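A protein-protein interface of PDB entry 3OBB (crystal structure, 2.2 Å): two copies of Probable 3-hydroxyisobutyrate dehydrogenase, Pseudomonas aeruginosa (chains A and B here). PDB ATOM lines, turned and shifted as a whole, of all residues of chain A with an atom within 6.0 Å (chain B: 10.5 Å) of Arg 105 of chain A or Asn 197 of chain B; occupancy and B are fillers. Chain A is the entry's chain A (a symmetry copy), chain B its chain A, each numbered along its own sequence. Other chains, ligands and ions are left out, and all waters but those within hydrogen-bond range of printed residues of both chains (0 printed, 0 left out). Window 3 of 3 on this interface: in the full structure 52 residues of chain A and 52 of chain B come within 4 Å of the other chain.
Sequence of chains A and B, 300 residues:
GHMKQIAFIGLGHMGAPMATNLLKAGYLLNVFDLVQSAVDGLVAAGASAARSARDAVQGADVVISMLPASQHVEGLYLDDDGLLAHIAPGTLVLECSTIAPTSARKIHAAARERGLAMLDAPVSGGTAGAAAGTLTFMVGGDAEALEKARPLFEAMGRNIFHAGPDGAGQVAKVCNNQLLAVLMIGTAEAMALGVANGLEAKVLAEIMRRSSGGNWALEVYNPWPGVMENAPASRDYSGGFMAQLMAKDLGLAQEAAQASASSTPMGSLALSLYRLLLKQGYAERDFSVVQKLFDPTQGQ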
ATOM      1  N   ALA A 100      -8.647 -14.059 -26.746  1.00  0.00           N
ATOM      2  CA  ALA A 100      -8.430 -12.635 -26.543  1.00  0.00           C
ATOM      3  C   ALA A 100      -9.729 -11.950 -26.077  1.00  0.00           C
ATOM      4  O   ALA A 100     -10.812 -12.250 -26.589  1.00  0.00           O
ATOM      5  CB  ALA A 100      -7.880 -11.993 -27.800  1.00  0.00           C
ATOM      6  N   PRO A 101      -9.634 -11.093 -25.045  1.00  0.00           N
ATOM      7  CA  PRO A 101     -10.766 -10.314 -24.582  1.00  0.00           C
ATOM      8  C   PRO A 101     -11.543  -9.614 -25.696  1.00  0.00           C
ATOM      9  O   PRO A 101     -12.767  -9.609 -25.647  1.00  0.00           O
ATOM     10  CB  PRO A 101     -10.110  -9.290 -23.649  1.00  0.00           C
ATOM     11  CG  PRO A 101      -9.013 -10.038 -23.058  1.00  0.00           C
ATOM     12  CD  PRO A 101      -8.462 -10.879 -24.172  1.00  0.00           C
ATOM     13  N   THR A 102     -10.840  -9.014 -26.661  1.00  0.00           N
ATOM     14  CA  THR A 102     -11.483  -8.331 -27.783  1.00  0.00           C
ATOM     15  C   THR A 102     -12.406  -9.337 -28.456  1.00  0.00           C
ATOM     16  O   THR A 102     -13.602  -9.090 -28.606  1.00  0.00           O
ATOM     17  CB  THR A 102     -10.469  -7.739 -28.807  1.00  0.00           C
ATOM     18  OG1 THR A 102      -9.706  -6.704 -28.182  1.00  0.00           O
ATOM     19  CG2 THR A 102     -11.192  -7.125 -29.997  1.00  0.00           C
ATOM     20  N   SER A 103     -11.847 -10.480 -28.827  1.00  0.00           N
ATOM     21  CA  SER A 103     -12.623 -11.560 -29.428  1.00  0.00           C
ATOM     22  C   SER A 103     -13.830 -12.016 -28.582  1.00  0.00           C
ATOM     23  O   SER A 103     -14.903 -12.254 -29.137  1.00  0.00           O
ATOM     24  CB  SER A 103     -11.716 -12.723 -29.795  1.00  0.00           C
ATOM     25  OG  SER A 103     -12.470 -13.890 -30.004  1.00  0.00           O
ATOM     26  N   ALA A 104     -13.672 -12.106 -27.262  1.00  0.00           N
ATOM     27  CA  ALA A 104     -14.800 -12.415 -26.363  1.00  0.00           C
ATOM     28  C   ALA A 104     -15.905 -11.356 -26.355  1.00  0.00           C
ATOM     29  O   ALA A 104     -17.083 -11.691 -26.218  1.00  0.00           O
ATOM     30  CB  ALA A 104     -14.313 -12.629 -24.954  1.00  0.00           C
ATOM     31  N   ARG A 105     -15.530 -10.085 -26.434  1.00  0.00           N
ATOM     32  CA  ARG A 105     -16.523  -9.003 -26.493  1.00  0.00           C
ATOM     33  C   ARG A 105     -17.313  -9.063 -27.795  1.00  0.00           C
ATOM     34  O   ARG A 105     -18.534  -8.860 -27.811  1.00  0.00           O
ATOM     35  CB  ARG A 105     -15.860  -7.626 -26.379  1.00  0.00           C
ATOM     36  CG  ARG A 105     -15.373  -7.321 -24.991  1.00  0.00           C
ATOM     37  CD  ARG A 105     -14.724  -5.961 -24.882  1.00  0.00           C
ATOM     38  NE  ARG A 105     -13.686  -6.095 -23.868  1.00  0.00           N
ATOM     39  CZ  ARG A 105     -12.382  -5.954 -24.080  1.00  0.00           C
ATOM     40  NH1 ARG A 105     -11.912  -5.593 -25.267  1.00  0.00           N
ATOM     41  NH2 ARG A 105     -11.559  -6.121 -23.065  1.00  0.00           N
ATOM     42  N   LYS A 106     -16.589  -9.307 -28.882  1.00  0.00           N
ATOM     43  CA  LYS A 106     -17.161  -9.472 -30.210  1.00  0.00           C
ATOM     44  C   LYS A 106     -18.221 -10.582 -30.211  1.00  0.00           C
ATOM     45  O   LYS A 106     -19.353 -10.364 -30.668  1.00  0.00           O
ATOM     46  CB  LYS A 106     -16.034  -9.755 -31.206  1.00  0.00           C
ATOM     47  CG  LYS A 106     -16.439  -9.730 -32.636  1.00  0.00           C
ATOM     48  CD  LYS A 106     -15.552  -8.775 -33.452  1.00  0.00           C
ATOM     49  CE  LYS A 106     -15.578  -9.165 -34.932  1.00  0.00           C
ATOM     50  NZ  LYS A 106     -15.154 -10.609 -35.089  1.00  0.00           N
ATOM     51  N   ILE A 107     -17.868 -11.758 -29.689  1.00  0.00           N
ATOM     52  CA  ILE A 107     -18.846 -12.831 -29.522  1.00  0.00           C
ATOM     53  C   ILE A 107     -19.967 -12.396 -28.572  1.00  0.00           C
ATOM     54  O   ILE A 107     -21.129 -12.636 -28.870  1.00  0.00           O
ATOM     55  CB  ILE A 107     -18.217 -14.191 -29.061  1.00  0.00           C
ATOM     56  CG1 ILE A 107     -17.195 -14.685 -30.091  1.00  0.00           C
ATOM     57  CG2 ILE A 107     -19.278 -15.265 -28.942  1.00  0.00           C
ATOM     58  CD1 ILE A 107     -16.067 -15.553 -29.508  1.00  0.00           C
ATOM     59  N   HIS A 108     -19.629 -11.765 -27.440  1.00  0.00           N
ATOM     60  CA  HIS A 108     -20.657 -11.310 -26.479  1.00  0.00           C
ATOM     61  C   HIS A 108     -21.743 -10.439 -27.129  1.00  0.00           C
ATOM     62  O   HIS A 108     -22.940 -10.634 -26.890  1.00  0.00           O
ATOM     63  CB  HIS A 108     -20.040 -10.526 -25.316  1.00  0.00           C
ATOM     64  CG  HIS A 108     -19.782 -11.349 -24.086  1.00  0.00           C
ATOM     65  ND1 HIS A 108     -20.782 -11.729 -23.222  1.00  0.00           N
ATOM     66  CD2 HIS A 108     -18.629 -11.812 -23.551  1.00  0.00           C
ATOM     67  CE1 HIS A 108     -20.264 -12.398 -22.212  1.00  0.00           C
ATOM     68  NE2 HIS A 108     -18.956 -12.465 -22.388  1.00  0.00           N
ATOM     69  N   ALA A 109     -21.304  -9.478 -27.943  1.00  0.00           N
ATOM     70  CA  ALA A 109     -22.188  -8.517 -28.590  1.00  0.00           C
ATOM     71  C   ALA A 109     -23.080  -9.191 -29.612  1.00  0.00           C
ATOM     72  O   ALA A 109     -24.275  -8.859 -29.729  1.00  0.00           O
ATOM     73  CB  ALA A 109     -21.376  -7.381 -29.255  1.00  0.00           C
ATOM     74  N   ALA A 110     -22.506 -10.118 -30.374  1.00  0.00           N
ATOM     75  CA  ALA A 110     -23.308 -10.845 -31.345  1.00  0.00           C
ATOM     76  C   ALA A 110     -24.360 -11.676 -30.602  1.00  0.00           C
ATOM     77  O   ALA A 110     -25.522 -11.672 -30.989  1.00  0.00           O
ATOM     78  CB  ALA A 110     -22.447 -11.691 -32.259  1.00  0.00           C
ATOM     79  N   ASP A 166     -18.831  -7.996 -19.796  1.00  0.00           N
ATOM     80  CA  ASP A 166     -18.472  -8.829 -20.936  1.00  0.00           C
ATOM     81  C   ASP A 166     -16.997  -8.766 -21.247  1.00  0.00           C
ATOM     82  O   ASP A 166     -16.463  -7.686 -21.375  1.00  0.00           O
ATOM     83  CB  ASP A 166     -19.244  -8.381 -22.168  1.00  0.00           C
ATOM     84  CG  ASP A 166     -20.707  -8.729 -22.097  1.00  0.00           C
ATOM     85  OD1 ASP A 166     -21.116  -9.482 -21.185  1.00  0.00           O
ATOM     86  OD2 ASP A 166     -21.437  -8.279 -22.983  1.00  0.00           O
ATOM     87  N   GLY A 167     -16.356  -9.932 -21.399  1.00  0.00           N
ATOM     88  CA  GLY A 167     -14.921  -9.997 -21.686  1.00  0.00           C
ATOM     89  C   GLY A 167     -13.971  -9.957 -20.488  1.00  0.00           C
ATOM     90  O   GLY A 167     -12.765 -10.226 -20.635  1.00  0.00           O
ATOM     91  N   ALA A 168     -14.505  -9.641 -19.304  1.00  0.00           N
ATOM     92  CA  ALA A 168     -13.692  -9.437 -18.084  1.00  0.00           C
ATOM     93  C   ALA A 168     -13.103 -10.729 -17.555  1.00  0.00           C
ATOM     94  O   ALA A 168     -12.050 -10.716 -16.898  1.00  0.00           O
ATOM     95  CB  ALA A 168     -14.504  -8.778 -17.012  1.00  0.00           C
ATOM     96  N   VAL A 171     -10.048 -11.073 -19.446  1.00  0.00           N
ATOM     97  CA  VAL A 171      -9.041 -10.094 -19.050  1.00  0.00           C
ATOM     98  C   VAL A 171      -8.346 -10.619 -17.796  1.00  0.00           C
ATOM     99  O   VAL A 171      -7.117 -10.612 -17.720  1.00  0.00           O
ATOM    100  CB  VAL A 171      -9.629  -8.625 -18.834  1.00  0.00           C
ATOM    101  CG1 VAL A 171      -8.557  -7.677 -18.395  1.00  0.00           C
ATOM    102  CG2 VAL A 171     -10.276  -8.078 -20.139  1.00  0.00           C
ATOM    103  N   ALA A 256      -4.095  -7.857 -25.503  1.00  0.00           N
ATOM    104  CA  ALA A 256      -4.799  -7.020 -24.526  1.00  0.00           C
ATOM    105  C   ALA A 256      -3.969  -5.790 -24.204  1.00  0.00           C
ATOM    106  O   ALA A 256      -4.517  -4.728 -24.060  1.00  0.00           O
ATOM    107  CB  ALA A 256      -5.139  -7.798 -23.259  1.00  0.00           C
ATOM    108  N   ALA A 257      -2.656  -5.938 -24.127  1.00  0.00           N
ATOM    109  CA  ALA A 257      -1.771  -4.811 -23.843  1.00  0.00           C
ATOM    110  C   ALA A 257      -1.773  -3.814 -25.009  1.00  0.00           C
ATOM    111  O   ALA A 257      -1.824  -2.604 -24.787  1.00  0.00           O
ATOM    112  CB  ALA A 257      -0.369  -5.295 -23.541  1.00  0.00           C
ATOM    113  N   ALA A 259      -4.159  -3.296 -27.020  1.00  0.00           N
ATOM    114  CA  ALA A 259      -5.501  -2.716 -27.062  1.00  0.00           C
ATOM    115  C   ALA A 259      -5.651  -1.572 -26.069  1.00  0.00           C
ATOM    116  O   ALA A 259      -6.421  -0.664 -26.307  1.00  0.00           O
ATOM    117  CB  ALA A 259      -6.581  -3.807 -26.820  1.00  0.00           C
ATOM    118  N   SER A 260      -4.897  -1.625 -24.968  1.00  0.00           N
ATOM    119  CA  SER A 260      -4.975  -0.602 -23.927  1.00  0.00           C
ATOM    120  C   SER A 260      -3.693   0.225 -23.795  1.00  0.00           C
ATOM    121  O   SER A 260      -3.597   1.075 -22.920  1.00  0.00           O
ATOM    122  CB  SER A 260      -5.281  -1.262 -22.601  1.00  0.00           C
ATOM    123  OG  SER A 260      -4.259  -2.185 -22.283  1.00  0.00           O
ATOM    124  N   SER A 262      -0.938  -0.738 -22.674  1.00  0.00           N
ATOM    125  CA  SER A 262      -0.307  -1.079 -21.418  1.00  0.00           C
ATOM    126  C   SER A 262       1.123  -1.596 -21.675  1.00  0.00           C
ATOM    127  O   SER A 262       1.349  -2.385 -22.585  1.00  0.00           O
ATOM    128  CB  SER A 262      -1.135  -2.137 -20.675  1.00  0.00           C
ATOM    129  OG  SER A 262      -2.466  -1.694 -20.474  1.00  0.00           O
ATOM    130  N   GLU B 189       2.380  -4.528 -13.166  1.00  0.00           N
ATOM    131  CA  GLU B 189       2.084  -4.495 -14.587  1.00  0.00           C
ATOM    132  C   GLU B 189       0.785  -5.254 -14.887  1.00  0.00           C
ATOM    133  O   GLU B 189       0.028  -4.868 -15.801  1.00  0.00           O
ATOM    134  CB  GLU B 189       3.270  -5.055 -15.398  1.00  0.00           C
ATOM    135  CG  GLU B 189       3.177  -6.503 -15.767  1.00  0.00           C
ATOM    136  CD  GLU B 189       4.399  -6.991 -16.610  1.00  0.00           C
ATOM    137  OE1 GLU B 189       5.359  -6.206 -16.809  1.00  0.00           O
ATOM    138  OE2 GLU B 189       4.362  -8.155 -17.077  1.00  0.00           O
ATOM    139  N   ALA B 190       0.544  -6.333 -14.133  1.00  0.00           N
ATOM    140  CA  ALA B 190      -0.688  -7.127 -14.298  1.00  0.00           C
ATOM    141  C   ALA B 190      -1.890  -6.307 -13.834  1.00  0.00           C
ATOM    142  O   ALA B 190      -2.895  -6.244 -14.536  1.00  0.00           O
ATOM    143  CB  ALA B 190      -0.593  -8.436 -13.530  1.00  0.00           C
ATOM    144  N   MET B 191      -1.777  -5.644 -12.686  1.00  0.00           N
ATOM    145  CA  MET B 191      -2.859  -4.789 -12.148  1.00  0.00           C
ATOM    146  C   MET B 191      -3.232  -3.689 -13.140  1.00  0.00           C
ATOM    147  O   MET B 191      -4.414  -3.428 -13.402  1.00  0.00           O
ATOM    148  CB  MET B 191      -2.437  -4.138 -10.808  1.00  0.00           C
ATOM    149  CG  MET B 191      -2.277  -5.112  -9.606  1.00  0.00           C
ATOM    150  SD  MET B 191      -3.965  -5.948  -9.097  1.00  0.00           S
ATOM    151  CE  MET B 191      -5.012  -4.329  -8.684  1.00  0.00           C
ATOM    152  N   ALA B 192      -2.218  -3.065 -13.721  1.00  0.00           N
ATOM    153  CA  ALA B 192      -2.417  -1.945 -14.647  1.00  0.00           C
ATOM    154  C   ALA B 192      -3.043  -2.432 -15.946  1.00  0.00           C
ATOM    155  O   ALA B 192      -3.957  -1.813 -16.482  1.00  0.00           O
ATOM    156  CB  ALA B 192      -1.069  -1.239 -14.907  1.00  0.00           C
ATOM    157  N   LEU B 193      -2.583  -3.586 -16.423  1.00  0.00           N
ATOM    158  CA  LEU B 193      -3.175  -4.186 -17.626  1.00  0.00           C
ATOM    159  C   LEU B 193      -4.697  -4.481 -17.420  1.00  0.00           C
ATOM    160  O   LEU B 193      -5.547  -4.113 -18.258  1.00  0.00           O
ATOM    161  CB  LEU B 193      -2.385  -5.439 -18.019  1.00  0.00           C
ATOM    162  CG  LEU B 193      -2.839  -6.240 -19.249  1.00  0.00           C
ATOM    163  CD1 LEU B 193      -2.959  -5.331 -20.515  1.00  0.00           C
ATOM    164  CD2 LEU B 193      -1.936  -7.476 -19.481  1.00  0.00           C
ATOM    165  N   GLY B 194      -5.025  -5.160 -16.316  1.00  0.00           N
ATOM    166  CA  GLY B 194      -6.427  -5.472 -16.007  1.00  0.00           C
ATOM    167  C   GLY B 194      -7.303  -4.222 -15.911  1.00  0.00           C
ATOM    168  O   GLY B 194      -8.354  -4.133 -16.573  1.00  0.00           O
ATOM    169  N   VAL B 195      -6.863  -3.255 -15.104  1.00  0.00           N
ATOM    170  CA  VAL B 195      -7.616  -2.007 -14.897  1.00  0.00           C
ATOM    171  C   VAL B 195      -7.771  -1.222 -16.218  1.00  0.00           C
ATOM    172  O   VAL B 195      -8.801  -0.599 -16.444  1.00  0.00           O
ATOM    173  CB  VAL B 195      -6.966  -1.107 -13.812  1.00  0.00           C
ATOM    174  CG1 VAL B 195      -7.740   0.229 -13.636  1.00  0.00           C
ATOM    175  CG2 VAL B 195      -6.939  -1.817 -12.511  1.00  0.00           C
ATOM    176  N   ALA B 196      -6.742  -1.262 -17.067  1.00  0.00           N
ATOM    177  CA  ALA B 196      -6.770  -0.567 -18.361  1.00  0.00           C
ATOM    178  C   ALA B 196      -7.767  -1.218 -19.306  1.00  0.00           C
ATOM    179  O   ALA B 196      -8.212  -0.590 -20.246  1.00  0.00           O
ATOM    180  CB  ALA B 196      -5.381  -0.562 -18.993  1.00  0.00           C
ATOM    181  N   ASN B 197      -8.114  -2.480 -19.030  1.00  0.00           N
ATOM    182  CA  ASN B 197      -8.994  -3.242 -19.862  1.00  0.00           C
ATOM    183  C   ASN B 197     -10.363  -3.398 -19.212  1.00  0.00           C
ATOM    184  O   ASN B 197     -11.136  -4.284 -19.592  1.00  0.00           O
ATOM    185  CB  ASN B 197      -8.354  -4.595 -20.201  1.00  0.00           C
ATOM    186  CG  ASN B 197      -7.374  -4.488 -21.367  1.00  0.00           C
ATOM    187  OD1 ASN B 197      -7.780  -4.400 -22.527  1.00  0.00           O
ATOM    188  ND2 ASN B 197      -6.091  -4.488 -21.068  1.00  0.00           N
ATOM    189  N   GLY B 198     -10.647  -2.522 -18.239  1.00  0.00           N
ATOM    190  CA  GLY B 198     -11.996  -2.369 -17.678  1.00  0.00           C
ATOM    191  C   GLY B 198     -12.305  -3.021 -16.327  1.00  0.00           C
ATOM    192  O   GLY B 198     -13.464  -3.006 -15.881  1.00  0.00           O
ATOM    193  N   LEU B 199     -11.295  -3.596 -15.670  1.00  0.00           N
ATOM    194  CA  LEU B 199     -11.520  -4.326 -14.409  1.00  0.00           C
ATOM    195  C   LEU B 199     -11.410  -3.442 -13.176  1.00  0.00           C
ATOM    196  O   LEU B 199     -10.666  -2.478 -13.179  1.00  0.00           O
ATOM    197  CB  LEU B 199     -10.530  -5.474 -14.267  1.00  0.00           C
ATOM    198  CG  LEU B 199     -10.928  -6.856 -14.801  1.00  0.00           C
ATOM    199  CD1 LEU B 199     -11.630  -6.804 -16.164  1.00  0.00           C
ATOM    200  CD2 LEU B 199      -9.682  -7.715 -14.870  1.00  0.00           C
ATOM    201  N   GLU B 200     -12.108  -3.804 -12.110  1.00  0.00           N
ATOM    202  CA  GLU B 200     -11.945  -3.117 -10.848  1.00  0.00           C
ATOM    203  C   GLU B 200     -10.705  -3.681 -10.197  1.00  0.00           C
ATOM    204  O   GLU B 200     -10.564  -4.911 -10.074  1.00  0.00           O
ATOM    205  CB  GLU B 200     -13.133  -3.389  -9.927  1.00  0.00           C
ATOM    206  CG  GLU B 200     -14.392  -2.656 -10.300  1.00  0.00           C
ATOM    207  CD  GLU B 200     -15.483  -2.910  -9.266  1.00  0.00           C
ATOM    208  OE1 GLU B 200     -16.516  -3.491  -9.640  1.00  0.00           O
ATOM    209  OE2 GLU B 200     -15.291  -2.566  -8.067  1.00  0.00           O
ATOM    210  N   ALA B 201      -9.825  -2.792  -9.735  1.00  0.00           N
ATOM    211  CA  ALA B 201      -8.533  -3.200  -9.195  1.00  0.00           C
ATOM    212  C   ALA B 201      -8.686  -4.265  -8.087  1.00  0.00           C
ATOM    213  O   ALA B 201      -7.976  -5.264  -8.108  1.00  0.00           O
ATOM    214  CB  ALA B 201      -7.754  -1.987  -8.703  1.00  0.00           C
ATOM    215  N   LEU B 204      -9.736  -7.818  -9.520  1.00  0.00           N
ATOM    216  CA  LEU B 204      -8.571  -8.431 -10.153  1.00  0.00           C
ATOM    217  C   LEU B 204      -7.513  -8.892  -9.145  1.00  0.00           C
ATOM    218  O   LEU B 204      -6.986 -10.002  -9.299  1.00  0.00           O
ATOM    219  CB  LEU B 204      -7.951  -7.500 -11.188  1.00  0.00           C
ATOM    220  CG  LEU B 204      -6.672  -8.035 -11.801  1.00  0.00           C
ATOM    221  CD1 LEU B 204      -6.892  -9.324 -12.663  1.00  0.00           C
ATOM    222  CD2 LEU B 204      -5.962  -6.954 -12.596  1.00  0.00           C
ATOM    223  N   TRP B 224      -1.207  -1.318  -6.084  1.00  0.00           N
ATOM    224  CA  TRP B 224      -2.287  -0.447  -6.622  1.00  0.00           C
ATOM    225  C   TRP B 224      -2.979   0.353  -5.525  1.00  0.00           C
ATOM    226  O   TRP B 224      -3.510  -0.246  -4.588  1.00  0.00           O
ATOM    227  CB  TRP B 224      -3.344  -1.261  -7.381  1.00  0.00           C
ATOM    228  CG  TRP B 224      -4.193  -0.369  -8.262  1.00  0.00           C
ATOM    229  CD1 TRP B 224      -5.344   0.278  -7.911  1.00  0.00           C
ATOM    230  CD2 TRP B 224      -3.935  -0.008  -9.619  1.00  0.00           C
ATOM    231  NE1 TRP B 224      -5.833   0.993  -8.978  1.00  0.00           N
ATOM    232  CE2 TRP B 224      -4.968   0.858 -10.029  1.00  0.00           C
ATOM    233  CE3 TRP B 224      -2.903  -0.296 -10.520  1.00  0.00           C
ATOM    234  CZ2 TRP B 224      -5.013   1.423 -11.312  1.00  0.00           C
ATOM    235  CZ3 TRP B 224      -2.953   0.264 -11.790  1.00  0.00           C
ATOM    236  CH2 TRP B 224      -3.998   1.120 -12.166  1.00  0.00           C
ATOM    237  N   PHE B 294       3.474   2.097 -14.807  1.00  0.00           N
ATOM    238  CA  PHE B 294       2.370   1.488 -15.576  1.00  0.00           C
ATOM    239  C   PHE B 294       1.030   2.189 -15.484  1.00  0.00           C
ATOM    240  O   PHE B 294       0.177   1.984 -16.356  1.00  0.00           O
ATOM    241  CB  PHE B 294       2.196   0.027 -15.161  1.00  0.00           C
ATOM    242  CG  PHE B 294       3.482  -0.725 -15.109  1.00  0.00           C
ATOM    243  CD1 PHE B 294       4.059  -1.045 -13.887  1.00  0.00           C
ATOM    244  CD2 PHE B 294       4.129  -1.080 -16.283  1.00  0.00           C
ATOM    245  CE1 PHE B 294       5.249  -1.736 -13.826  1.00  0.00           C
ATOM    246  CE2 PHE B 294       5.340  -1.763 -16.239  1.00  0.00           C
ATOM    247  CZ  PHE B 294       5.901  -2.084 -15.004  1.00  0.00           C
ATOM    248  N   PRO B 296      -1.167   5.429 -15.493  1.00  0.00           N
ATOM    249  CA  PRO B 296      -1.121   6.790 -16.033  1.00  0.00           C
ATOM    250  C   PRO B 296      -1.846   7.809 -15.158  1.00  0.00           C
ATOM    251  O   PRO B 296      -1.533   8.997 -15.206  1.00  0.00           O
ATOM    252  CB  PRO B 296      -1.834   6.652 -17.377  1.00  0.00           C
ATOM    253  CG  PRO B 296      -2.823   5.491 -17.180  1.00  0.00           C
ATOM    254  CD  PRO B 296      -2.116   4.554 -16.227  1.00  0.00           C
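Printed residues of chain B that touch a printed residue of chain A: Leu 193, Gly 194, Ala 196, Asn 197 and Leu 199.
Hydrophobic or aromatic side chains of chain A within 4 Å of the printed part of chain B: Ala 168, Val 171 and Ala 257.
Among the printed residues, 13 pairs touch across the chains.
Among the printed residues, no Asp or Glu carboxylate lies within 4 Å of a Lys or Arg side-chain nitrogen of the other chain.
The backbone carbonyl oxygen of Gly 194 of chain B sits at hydrogen-bond distance from the backbone NH of Leu 199 of chain B, 3.1 Å away.
The backbone carbonyl oxygen (O) of Leu 193 of chain B lies within hydrogen-bond range of the side-chain amide nitrogen (ND2) of Asn 197 of chain B, at 2.9 Å.
OG of Ser 260 of chain A is in hydrogen-bond range of OG of Ser 262 of chain A (2.6 Å).
The side-chain hydroxyl (OG) of Ser 260 of chain A is in hydrogen-bond range of the backbone carbonyl oxygen (O) of Ala 256 of chain A (3.1 Å).
N of Ser 262 of chain A is in hydrogen-bond range of O of Ala 257 of chain A, 3.0 Å away.
Arg 105 of chain A touches just one residue of chain B: Asn 197 (3.95 Å).
Asn 197 of chain B touches four residues of chain A.
No residue of chain B comes within 4 Å of Thr 102 of chain A.
No residue of chain B comes within 4 Å of Ala 109 of chain A.
No residue of chain B comes within 4 Å of Gly 167 of chain A.
Ala 257 of chain A touches one residue of chain B.
Ser 260 of chain A touches three residues of chain B.
Printed residues of chain A within 4 Å of Gly 194 of chain B: Val 171 (3.9 Å).
Of the printed residues of chain B, Ala 168 of chain A touches Leu 199.
Of the printed residues of chain A, Leu 199 of chain B touches Ala 168 (3.6 Å) and Val 171 (3.7 Å).
Printed residues of chain A within 4 Å of Leu 193 of chain B: Ala 256 (3.9 Å), Ala 257 (3.6 Å), Ser 260 (3.8 Å) and Ser 262 (3.7 Å).
Of the printed residues of chain B, Ser 262 of chain A touches Leu 193 (3.7 Å) and Ala 196 (3.5 Å).
Among the printed residues, merely in contact across the chains: Ser 262 of chain A with Ala 196 of chain B (3.5 Å), Ala 257 of chain A with Leu 193 of chain B (3.6 Å), Val 171 of chain A with Asn 197 of chain B (3.6 Å), Ala 168 of chain A with Leu 199 of chain B (3.6 Å), Ser 262 of chain A with Leu 193 of chain B (3.7 Å), Ser 260 of chain A with Ala 196 of chain B (3.7 Å), Val 171 of chain A with Leu 199 of chain B (3.7 Å), Ser 260 of chain A with Leu 193 of chain B (3.8 Å), Ala 256 of chain A with Leu 193 of chain B (3.9 Å), Val 171 of chain A with Gly 194 of chain B (3.9 Å) and Arg 105 of chain A with Asn 197 of chain B (3.95 Å).
The side-chain amide nitrogen (ND2) of Asn 197 of chain B lies within hydrogen-bond range of the side-chain hydroxyl (OG) of Ser 260 of chain A, 3.2 Å away.
The backbone carbonyl oxygen of Ala 256 of chain A sits at hydrogen-bond distance from the side-chain amide nitrogen of Asn 197 of chain B (3.4 Å).
No position is printed for both chains.
Of the 13 pairs that touch across the chains among the printed residues, none has its exchanged pair printed and touching as well.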
